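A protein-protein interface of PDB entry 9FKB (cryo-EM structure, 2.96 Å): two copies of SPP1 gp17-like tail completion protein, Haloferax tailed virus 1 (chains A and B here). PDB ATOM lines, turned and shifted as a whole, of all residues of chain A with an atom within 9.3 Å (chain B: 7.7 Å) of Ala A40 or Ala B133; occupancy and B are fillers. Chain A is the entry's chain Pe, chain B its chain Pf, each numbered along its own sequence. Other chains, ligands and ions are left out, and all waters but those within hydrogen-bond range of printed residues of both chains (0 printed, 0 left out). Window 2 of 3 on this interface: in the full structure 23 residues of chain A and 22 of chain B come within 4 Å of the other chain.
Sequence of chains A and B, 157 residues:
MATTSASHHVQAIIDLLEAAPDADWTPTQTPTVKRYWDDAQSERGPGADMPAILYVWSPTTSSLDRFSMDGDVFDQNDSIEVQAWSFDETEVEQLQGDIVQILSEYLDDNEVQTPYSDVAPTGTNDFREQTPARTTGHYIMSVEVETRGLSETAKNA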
ATOM      1  N   LYS A  34      19.719  26.276  18.394  1.00  0.00           N
ATOM      2  CA  LYS A  34      19.920  26.783  17.041  1.00  0.00           C
ATOM      3  C   LYS A  34      18.687  26.541  16.173  1.00  0.00           C
ATOM      4  O   LYS A  34      17.939  25.600  16.406  1.00  0.00           O
ATOM      5  CB  LYS A  34      21.096  26.041  16.408  1.00  0.00           C
ATOM      6  CG  LYS A  34      22.451  26.479  16.939  1.00  0.00           C
ATOM      7  CD  LYS A  34      23.609  25.919  16.139  1.00  0.00           C
ATOM      8  CE  LYS A  34      24.908  26.620  16.474  1.00  0.00           C
ATOM      9  NZ  LYS A  34      26.038  26.136  15.648  1.00  0.00           N
ATOM     10  N   ARG A  35      18.492  27.357  15.130  1.00  0.00           N
ATOM     11  CA  ARG A  35      17.584  26.967  14.054  1.00  0.00           C
ATOM     12  C   ARG A  35      18.232  25.830  13.272  1.00  0.00           C
ATOM     13  O   ARG A  35      19.452  25.791  13.161  1.00  0.00           O
ATOM     14  CB  ARG A  35      17.280  28.127  13.099  1.00  0.00           C
ATOM     15  CG  ARG A  35      16.630  29.343  13.747  1.00  0.00           C
ATOM     16  CD  ARG A  35      17.581  30.214  14.561  1.00  0.00           C
ATOM     17  NE  ARG A  35      17.261  31.619  14.385  1.00  0.00           N
ATOM     18  CZ  ARG A  35      17.681  32.372  13.372  1.00  0.00           C
ATOM     19  NH1 ARG A  35      17.315  33.638  13.306  1.00  0.00           N
ATOM     20  NH2 ARG A  35      18.466  31.880  12.431  1.00  0.00           N
ATOM     21  N   TYR A  36      17.442  24.944  12.668  1.00  0.00           N
ATOM     22  CA  TYR A  36      18.009  23.840  11.899  1.00  0.00           C
ATOM     23  C   TYR A  36      18.939  24.338  10.795  1.00  0.00           C
ATOM     24  O   TYR A  36      19.963  23.719  10.518  1.00  0.00           O
ATOM     25  CB  TYR A  36      16.891  22.981  11.328  1.00  0.00           C
ATOM     26  CG  TYR A  36      17.306  21.759  10.549  1.00  0.00           C
ATOM     27  CD1 TYR A  36      17.507  20.534  11.179  1.00  0.00           C
ATOM     28  CD2 TYR A  36      17.455  21.813   9.167  1.00  0.00           C
ATOM     29  CE1 TYR A  36      17.848  19.396  10.449  1.00  0.00           C
ATOM     30  CE2 TYR A  36      17.778  20.681   8.425  1.00  0.00           C
ATOM     31  CZ  TYR A  36      17.972  19.463   9.064  1.00  0.00           C
ATOM     32  OH  TYR A  36      18.293  18.347   8.327  1.00  0.00           O
ATOM     33  N   TRP A  37      18.596  25.475  10.182  1.00  0.00           N
ATOM     34  CA  TRP A  37      19.350  26.070   9.087  1.00  0.00           C
ATOM     35  C   TRP A  37      20.566  26.922   9.499  1.00  0.00           C
ATOM     36  O   TRP A  37      21.215  27.512   8.630  1.00  0.00           O
ATOM     37  CB  TRP A  37      18.363  26.856   8.224  1.00  0.00           C
ATOM     38  CG  TRP A  37      17.758  28.066   8.872  1.00  0.00           C
ATOM     39  CD1 TRP A  37      18.314  29.309   8.905  1.00  0.00           C
ATOM     40  CD2 TRP A  37      16.470  28.193   9.535  1.00  0.00           C
ATOM     41  NE1 TRP A  37      17.467  30.190   9.523  1.00  0.00           N
ATOM     42  CE2 TRP A  37      16.324  29.547   9.931  1.00  0.00           C
ATOM     43  CE3 TRP A  37      15.423  27.309   9.843  1.00  0.00           C
ATOM     44  CZ2 TRP A  37      15.183  30.023  10.603  1.00  0.00           C
ATOM     45  CZ3 TRP A  37      14.297  27.770  10.504  1.00  0.00           C
ATOM     46  CH2 TRP A  37      14.185  29.112  10.881  1.00  0.00           C
ATOM     47  N   ASP A  38      20.916  27.001  10.790  1.00  0.00           N
ATOM     48  CA  ASP A  38      22.092  27.752  11.226  1.00  0.00           C
ATOM     49  C   ASP A  38      23.417  27.081  10.822  1.00  0.00           C
ATOM     50  O   ASP A  38      24.428  27.767  10.674  1.00  0.00           O
ATOM     51  CB  ASP A  38      22.061  27.993  12.737  1.00  0.00           C
ATOM     52  CG  ASP A  38      21.028  28.978  13.258  1.00  0.00           C
ATOM     53  OD1 ASP A  38      20.549  29.828  12.464  1.00  0.00           O
ATOM     54  OD2 ASP A  38      20.740  28.919  14.482  1.00  0.00           O
ATOM     55  N   ASP A  39      23.425  25.749  10.628  1.00  0.00           N
ATOM     56  CA  ASP A  39      24.622  24.959  10.334  1.00  0.00           C
ATOM     57  C   ASP A  39      24.511  24.205   9.002  1.00  0.00           C
ATOM     58  O   ASP A  39      23.437  23.755   8.623  1.00  0.00           O
ATOM     59  CB  ASP A  39      24.891  23.949  11.456  1.00  0.00           C
ATOM     60  CG  ASP A  39      25.171  24.530  12.837  1.00  0.00           C
ATOM     61  OD1 ASP A  39      25.483  25.733  12.965  1.00  0.00           O
ATOM     62  OD2 ASP A  39      25.120  23.744  13.805  1.00  0.00           O
ATOM     63  N   ALA A  40      25.639  24.026   8.295  1.00  0.00           N
ATOM     64  CA  ALA A  40      25.679  23.140   7.131  1.00  0.00           C
ATOM     65  C   ALA A  40      25.787  21.680   7.580  1.00  0.00           C
ATOM     66  O   ALA A  40      26.275  21.387   8.669  1.00  0.00           O
ATOM     67  CB  ALA A  40      26.814  23.489   6.190  1.00  0.00           C
ATOM     68  N   GLN A  41      25.387  20.752   6.706  1.00  0.00           N
ATOM     69  CA  GLN A  41      25.182  19.360   7.097  1.00  0.00           C
ATOM     70  C   GLN A  41      26.448  18.690   7.650  1.00  0.00           C
ATOM     71  O   GLN A  41      26.395  17.978   8.655  1.00  0.00           O
ATOM     72  CB  GLN A  41      24.578  18.584   5.931  1.00  0.00           C
ATOM     73  CG  GLN A  41      24.155  17.166   6.305  1.00  0.00           C
ATOM     74  CD  GLN A  41      23.035  17.139   7.327  1.00  0.00           C
ATOM     75  OE1 GLN A  41      23.222  17.394   8.523  1.00  0.00           O
ATOM     76  NE2 GLN A  41      21.834  16.808   6.870  1.00  0.00           N
ATOM     77  N   SER A  42      27.608  18.928   7.024  1.00  0.00           N
ATOM     78  CA  SER A  42      28.878  18.352   7.470  1.00  0.00           C
ATOM     79  C   SER A  42      29.339  18.891   8.828  1.00  0.00           C
ATOM     80  O   SER A  42      30.105  18.225   9.537  1.00  0.00           O
ATOM     81  CB  SER A  42      29.954  18.555   6.448  1.00  0.00           C
ATOM     82  OG  SER A  42      29.481  18.157   5.184  1.00  0.00           O
ATOM     83  N   GLU A  43      28.886  20.106   9.180  1.00  0.00           N
ATOM     84  CA  GLU A  43      29.177  20.736  10.463  1.00  0.00           C
ATOM     85  C   GLU A  43      28.130  20.393  11.526  1.00  0.00           C
ATOM     86  O   GLU A  43      28.422  20.577  12.708  1.00  0.00           O
ATOM     87  CB  GLU A  43      29.271  22.256  10.301  1.00  0.00           C
ATOM     88  CG  GLU A  43      30.658  22.782   9.951  1.00  0.00           C
ATOM     89  CD  GLU A  43      31.020  22.753   8.477  1.00  0.00           C
ATOM     90  OE1 GLU A  43      31.002  21.664   7.869  1.00  0.00           O
ATOM     91  OE2 GLU A  43      31.338  23.828   7.939  1.00  0.00           O
ATOM     92  N   ARG A  44      26.939  19.913  11.128  1.00  0.00           N
ATOM     93  CA  ARG A  44      25.799  19.726  12.015  1.00  0.00           C
ATOM     94  C   ARG A  44      26.109  18.726  13.138  1.00  0.00           C
ATOM     95  O   ARG A  44      26.807  17.726  12.937  1.00  0.00           O
ATOM     96  CB  ARG A  44      24.553  19.354  11.198  1.00  0.00           C
ATOM     97  CG  ARG A  44      23.268  19.432  12.011  1.00  0.00           C
ATOM     98  CD  ARG A  44      21.990  19.281  11.210  1.00  0.00           C
ATOM     99  NE  ARG A  44      21.582  20.505  10.553  1.00  0.00           N
ATOM    100  CZ  ARG A  44      21.425  20.685   9.239  1.00  0.00           C
ATOM    101  NH1 ARG A  44      20.995  21.840   8.775  1.00  0.00           N
ATOM    102  NH2 ARG A  44      21.675  19.731   8.367  1.00  0.00           N
ATOM    103  N   GLY A  45      25.542  19.007  14.323  1.00  0.00           N
ATOM    104  CA  GLY A  45      25.871  18.311  15.556  1.00  0.00           C
ATOM    105  C   GLY A  45      27.106  18.895  16.234  1.00  0.00           C
ATOM    106  O   GLY A  45      27.905  19.582  15.609  1.00  0.00           O
ATOM    107  N   TYR A  55      18.383  21.623  17.598  1.00  0.00           N
ATOM    108  CA  TYR A  55      17.938  22.243  16.355  1.00  0.00           C
ATOM    109  C   TYR A  55      16.414  22.341  16.318  1.00  0.00           C
ATOM    110  O   TYR A  55      15.725  21.347  16.495  1.00  0.00           O
ATOM    111  CB  TYR A  55      18.445  21.462  15.143  1.00  0.00           C
ATOM    112  CG  TYR A  55      19.943  21.488  14.998  1.00  0.00           C
ATOM    113  CD1 TYR A  55      20.607  22.635  14.596  1.00  0.00           C
ATOM    114  CD2 TYR A  55      20.701  20.363  15.286  1.00  0.00           C
ATOM    115  CE1 TYR A  55      21.988  22.670  14.471  1.00  0.00           C
ATOM    116  CE2 TYR A  55      22.085  20.379  15.170  1.00  0.00           C
ATOM    117  CZ  TYR A  55      22.729  21.534  14.756  1.00  0.00           C
ATOM    118  OH  TYR A  55      24.098  21.545  14.646  1.00  0.00           O
ATOM    119  N   TRP A  85      21.189  16.631  19.285  1.00  0.00           N
ATOM    120  CA  TRP A  85      22.338  15.880  18.793  1.00  0.00           C
ATOM    121  C   TRP A  85      23.445  15.836  19.858  1.00  0.00           C
ATOM    122  O   TRP A  85      23.878  16.873  20.352  1.00  0.00           O
ATOM    123  CB  TRP A  85      22.887  16.530  17.513  1.00  0.00           C
ATOM    124  CG  TRP A  85      22.046  16.536  16.267  1.00  0.00           C
ATOM    125  CD1 TRP A  85      20.732  16.874  16.135  1.00  0.00           C
ATOM    126  CD2 TRP A  85      22.497  16.234  14.919  1.00  0.00           C
ATOM    127  NE1 TRP A  85      20.344  16.774  14.820  1.00  0.00           N
ATOM    128  CE2 TRP A  85      21.412  16.417  14.033  1.00  0.00           C
ATOM    129  CE3 TRP A  85      23.725  15.843  14.359  1.00  0.00           C
ATOM    130  CZ2 TRP A  85      21.538  16.220  12.644  1.00  0.00           C
ATOM    131  CZ3 TRP A  85      23.858  15.634  12.993  1.00  0.00           C
ATOM    132  CH2 TRP A  85      22.770  15.836  12.138  1.00  0.00           C
ATOM    133  N   HIS A 138      26.925  11.120  15.760  1.00  0.00           N
ATOM    134  CA  HIS A 138      25.832  11.650  16.558  1.00  0.00           C
ATOM    135  C   HIS A 138      24.699  10.648  16.730  1.00  0.00           C
ATOM    136  O   HIS A 138      24.229  10.061  15.766  1.00  0.00           O
ATOM    137  CB  HIS A 138      25.327  12.951  15.942  1.00  0.00           C
ATOM    138  CG  HIS A 138      26.409  13.976  15.885  1.00  0.00           C
ATOM    139  ND1 HIS A 138      27.041  14.372  14.704  1.00  0.00           N
ATOM    140  CD2 HIS A 138      27.000  14.651  16.885  1.00  0.00           C
ATOM    141  CE1 HIS A 138      27.964  15.261  14.996  1.00  0.00           C
ATOM    142  NE2 HIS A 138      27.958  15.449  16.330  1.00  0.00           N
ATOM    143  N   GLU B 129      14.394  25.696   6.817  1.00  0.00           N
ATOM    144  CA  GLU B 129      15.237  24.550   7.139  1.00  0.00           C
ATOM    145  C   GLU B 129      15.976  23.979   5.919  1.00  0.00           C
ATOM    146  O   GLU B 129      16.980  23.282   6.085  1.00  0.00           O
ATOM    147  CB  GLU B 129      14.425  23.462   7.850  1.00  0.00           C
ATOM    148  CG  GLU B 129      13.536  22.597   6.951  1.00  0.00           C
ATOM    149  CD  GLU B 129      12.260  23.214   6.392  1.00  0.00           C
ATOM    150  OE1 GLU B 129      11.965  24.357   6.779  1.00  0.00           O
ATOM    151  OE2 GLU B 129      11.587  22.567   5.562  1.00  0.00           O
ATOM    152  N   GLN B 130      15.509  24.283   4.703  1.00  0.00           N
ATOM    153  CA  GLN B 130      15.993  23.639   3.488  1.00  0.00           C
ATOM    154  C   GLN B 130      17.156  24.383   2.841  1.00  0.00           C
ATOM    155  O   GLN B 130      17.939  23.779   2.113  1.00  0.00           O
ATOM    156  CB  GLN B 130      14.857  23.493   2.487  1.00  0.00           C
ATOM    157  CG  GLN B 130      13.641  22.847   3.131  1.00  0.00           C
ATOM    158  CD  GLN B 130      12.584  22.403   2.153  1.00  0.00           C
ATOM    159  OE1 GLN B 130      12.761  22.473   0.936  1.00  0.00           O
ATOM    160  NE2 GLN B 130      11.466  21.940   2.700  1.00  0.00           N
ATOM    161  N   THR B 131      17.272  25.687   3.095  1.00  0.00           N
ATOM    162  CA  THR B 131      18.375  26.495   2.594  1.00  0.00           C
ATOM    163  C   THR B 131      19.668  26.026   3.265  1.00  0.00           C
ATOM    164  O   THR B 131      19.765  26.046   4.490  1.00  0.00           O
ATOM    165  CB  THR B 131      18.125  27.979   2.898  1.00  0.00           C
ATOM    166  OG1 THR B 131      16.810  28.339   2.470  1.00  0.00           O
ATOM    167  CG2 THR B 131      19.110  28.907   2.219  1.00  0.00           C
ATOM    168  N   PRO B 132      20.711  25.593   2.509  1.00  0.00           N
ATOM    169  CA  PRO B 132      21.968  25.151   3.127  1.00  0.00           C
ATOM    170  C   PRO B 132      22.776  26.353   3.635  1.00  0.00           C
ATOM    171  O   PRO B 132      22.650  27.463   3.118  1.00  0.00           O
ATOM    172  CB  PRO B 132      22.681  24.411   1.984  1.00  0.00           C
ATOM    173  CG  PRO B 132      22.156  25.086   0.724  1.00  0.00           C
ATOM    174  CD  PRO B 132      20.728  25.482   1.037  1.00  0.00           C
ATOM    175  N   ALA B 133      23.627  26.134   4.647  1.00  0.00           N
ATOM    176  CA  ALA B 133      24.244  27.243   5.378  1.00  0.00           C
ATOM    177  C   ALA B 133      25.550  27.788   4.762  1.00  0.00           C
ATOM    178  O   ALA B 133      25.925  28.937   5.037  1.00  0.00           O
ATOM    179  CB  ALA B 133      24.401  26.889   6.836  1.00  0.00           C
ATOM    180  N   ARG B 134      26.258  26.996   3.931  1.00  0.00           N
ATOM    181  CA  ARG B 134      27.520  27.409   3.312  1.00  0.00           C
ATOM    182  C   ARG B 134      27.308  28.545   2.313  1.00  0.00           C
ATOM    183  O   ARG B 134      27.944  29.596   2.427  1.00  0.00           O
ATOM    184  CB  ARG B 134      28.167  26.269   2.516  1.00  0.00           C
ATOM    185  CG  ARG B 134      28.710  25.117   3.340  1.00  0.00           C
ATOM    186  CD  ARG B 134      29.780  24.338   2.604  1.00  0.00           C
ATOM    187  NE  ARG B 134      30.146  23.258   3.494  1.00  0.00           N
ATOM    188  CZ  ARG B 134      31.059  23.317   4.464  1.00  0.00           C
ATOM    189  NH1 ARG B 134      31.285  22.246   5.203  1.00  0.00           N
ATOM    190  NH2 ARG B 134      31.746  24.424   4.698  1.00  0.00           N
ATOM    191  N   THR B 135      26.501  28.254   1.284  1.00  0.00           N
ATOM    192  CA  THR B 135      26.216  29.146   0.173  1.00  0.00           C
ATOM    193  C   THR B 135      25.138  30.136   0.596  1.00  0.00           C
ATOM    194  O   THR B 135      24.118  29.737   1.140  1.00  0.00           O
ATOM    195  CB  THR B 135      25.673  28.361  -1.035  1.00  0.00           C
ATOM    196  OG1 THR B 135      24.619  27.504  -0.592  1.00  0.00           O
ATOM    197  CG2 THR B 135      26.716  27.574  -1.801  1.00  0.00           C
ATOM    198  N   THR B 136      25.313  31.423   0.276  1.00  0.00           N
ATOM    199  CA  THR B 136      24.158  32.309   0.275  1.00  0.00           C
ATOM    200  C   THR B 136      23.142  31.793  -0.756  1.00  0.00           C
ATOM    201  O   THR B 136      23.512  31.341  -1.838  1.00  0.00           O
ATOM    202  CB  THR B 136      24.575  33.775   0.101  1.00  0.00           C
ATOM    203  OG1 THR B 136      23.462  34.634   0.361  1.00  0.00           O
ATOM    204  CG2 THR B 136      25.093  34.060  -1.289  1.00  0.00           C
ATOM    205  N   GLY B 137      21.855  31.843  -0.397  1.00  0.00           N
ATOM    206  CA  GLY B 137      20.775  31.277  -1.189  1.00  0.00           C
ATOM    207  C   GLY B 137      19.431  31.716  -0.620  1.00  0.00           C
ATOM    208  O   GLY B 137      19.371  32.251   0.486  1.00  0.00           O
ATOM    209  N   TYR B 139      16.118  31.915   1.266  1.00  0.00           N
ATOM    210  CA  TYR B 139      15.123  31.421   2.200  1.00  0.00           C
ATOM    211  C   TYR B 139      13.750  31.490   1.531  1.00  0.00           C
ATOM    212  O   TYR B 139      13.488  32.403   0.749  1.00  0.00           O
ATOM    213  CB  TYR B 139      15.178  32.247   3.485  1.00  0.00           C
ATOM    214  CG  TYR B 139      16.490  32.077   4.203  1.00  0.00           C
ATOM    215  CD1 TYR B 139      16.804  30.876   4.828  1.00  0.00           C
ATOM    216  CD2 TYR B 139      17.441  33.086   4.202  1.00  0.00           C
ATOM    217  CE1 TYR B 139      18.040  30.679   5.434  1.00  0.00           C
ATOM    218  CE2 TYR B 139      18.683  32.898   4.798  1.00  0.00           C
ATOM    219  CZ  TYR B 139      18.987  31.693   5.420  1.00  0.00           C
ATOM    220  OH  TYR B 139      20.200  31.517   6.038  1.00  0.00           O
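OD2 of Asp A39 lies within hydrogen-bond range of OH of Tyr A55 (2.6 Å). The guanidinium group (NH2) of Arg A35 lies within salt-bridge range of the side-chain carboxylate (OD1) of Asp A38, 2.9 Å away. The side-chain amino group of Lys A34 lies within salt-bridge range of the side-chain carboxylate of Asp A39, at 2.8 Å. The side-chain carboxylate of Glu B129 lies within hydrogen-bond range of the side-chain amide nitrogen of Gln B130. O of Tyr A36 sits at hydrogen-bond distance from NH1 of Arg A44 (2.8 Å). NH1 of Arg A44 is in hydrogen-bond range of O of Asp A39.
The side-chain carboxylate (OE1) of Glu A43 lies within salt-bridge range of the guanidinium group (NH1) of Arg B134.
No position is printed for both chains.
Ala A40 touches just these residues of chain B: Ala B133 and Arg B134. Ala B133 touches just these residues of chain A: Trp A37 (3.7 Å), Asp A38 (3.9 Å), Asp A39 (3.5 Å) and Ala A40 (3.4 Å). No residue of chain A comes within 4 Å of Pro B132. Arg B134 touches just these residues of chain A: Ala A40 and Glu A43. Of the printed residues of chain B, Tyr A36 touches Glu B129. Printed residues of chain B within 4 Å of Asp A38: Ala B133. Of the printed residues of chain B, Asp A39 touches Ala B133. Of the printed residues of chain B, Glu A43 touches Arg B134 (2.7 Å). Printed residues of chain B within 4 Å of Trp A37: Glu B129, Ala B133 and Tyr B139. The nearest residue of chain B that does not touch Ala A40 is Pro B132 (5.6 Å). The nearest residue of chain A that does not touch Ala B133 is Gln A41 (6.0 Å).
Printed residues of chain B that touch a printed residue of chain A: Glu B129, Ala B133, Arg B134 and Tyr B139. Hydrophobic or aromatic side chains of chain B that line the printed part of chain A: Ala B133 and Tyr B139. Among the printed residues, 9 pairs touch across the chains.
Among the printed residues, merely in contact across the chains: Tyr A36 with Glu B129 (3.4 Å), Trp A37 with Glu B129 (3.6 Å), Trp A37 with Ala B133 (3.7 Å), Trp A37 with Tyr B139 (3.7 Å), Asp A38 with Ala B133 (3.9 Å), Asp A39 with Ala B133 (3.5 Å), Ala A40 with Ala B133 (3.4 Å) and Ala A40 with Arg B134 (3.8 Å).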
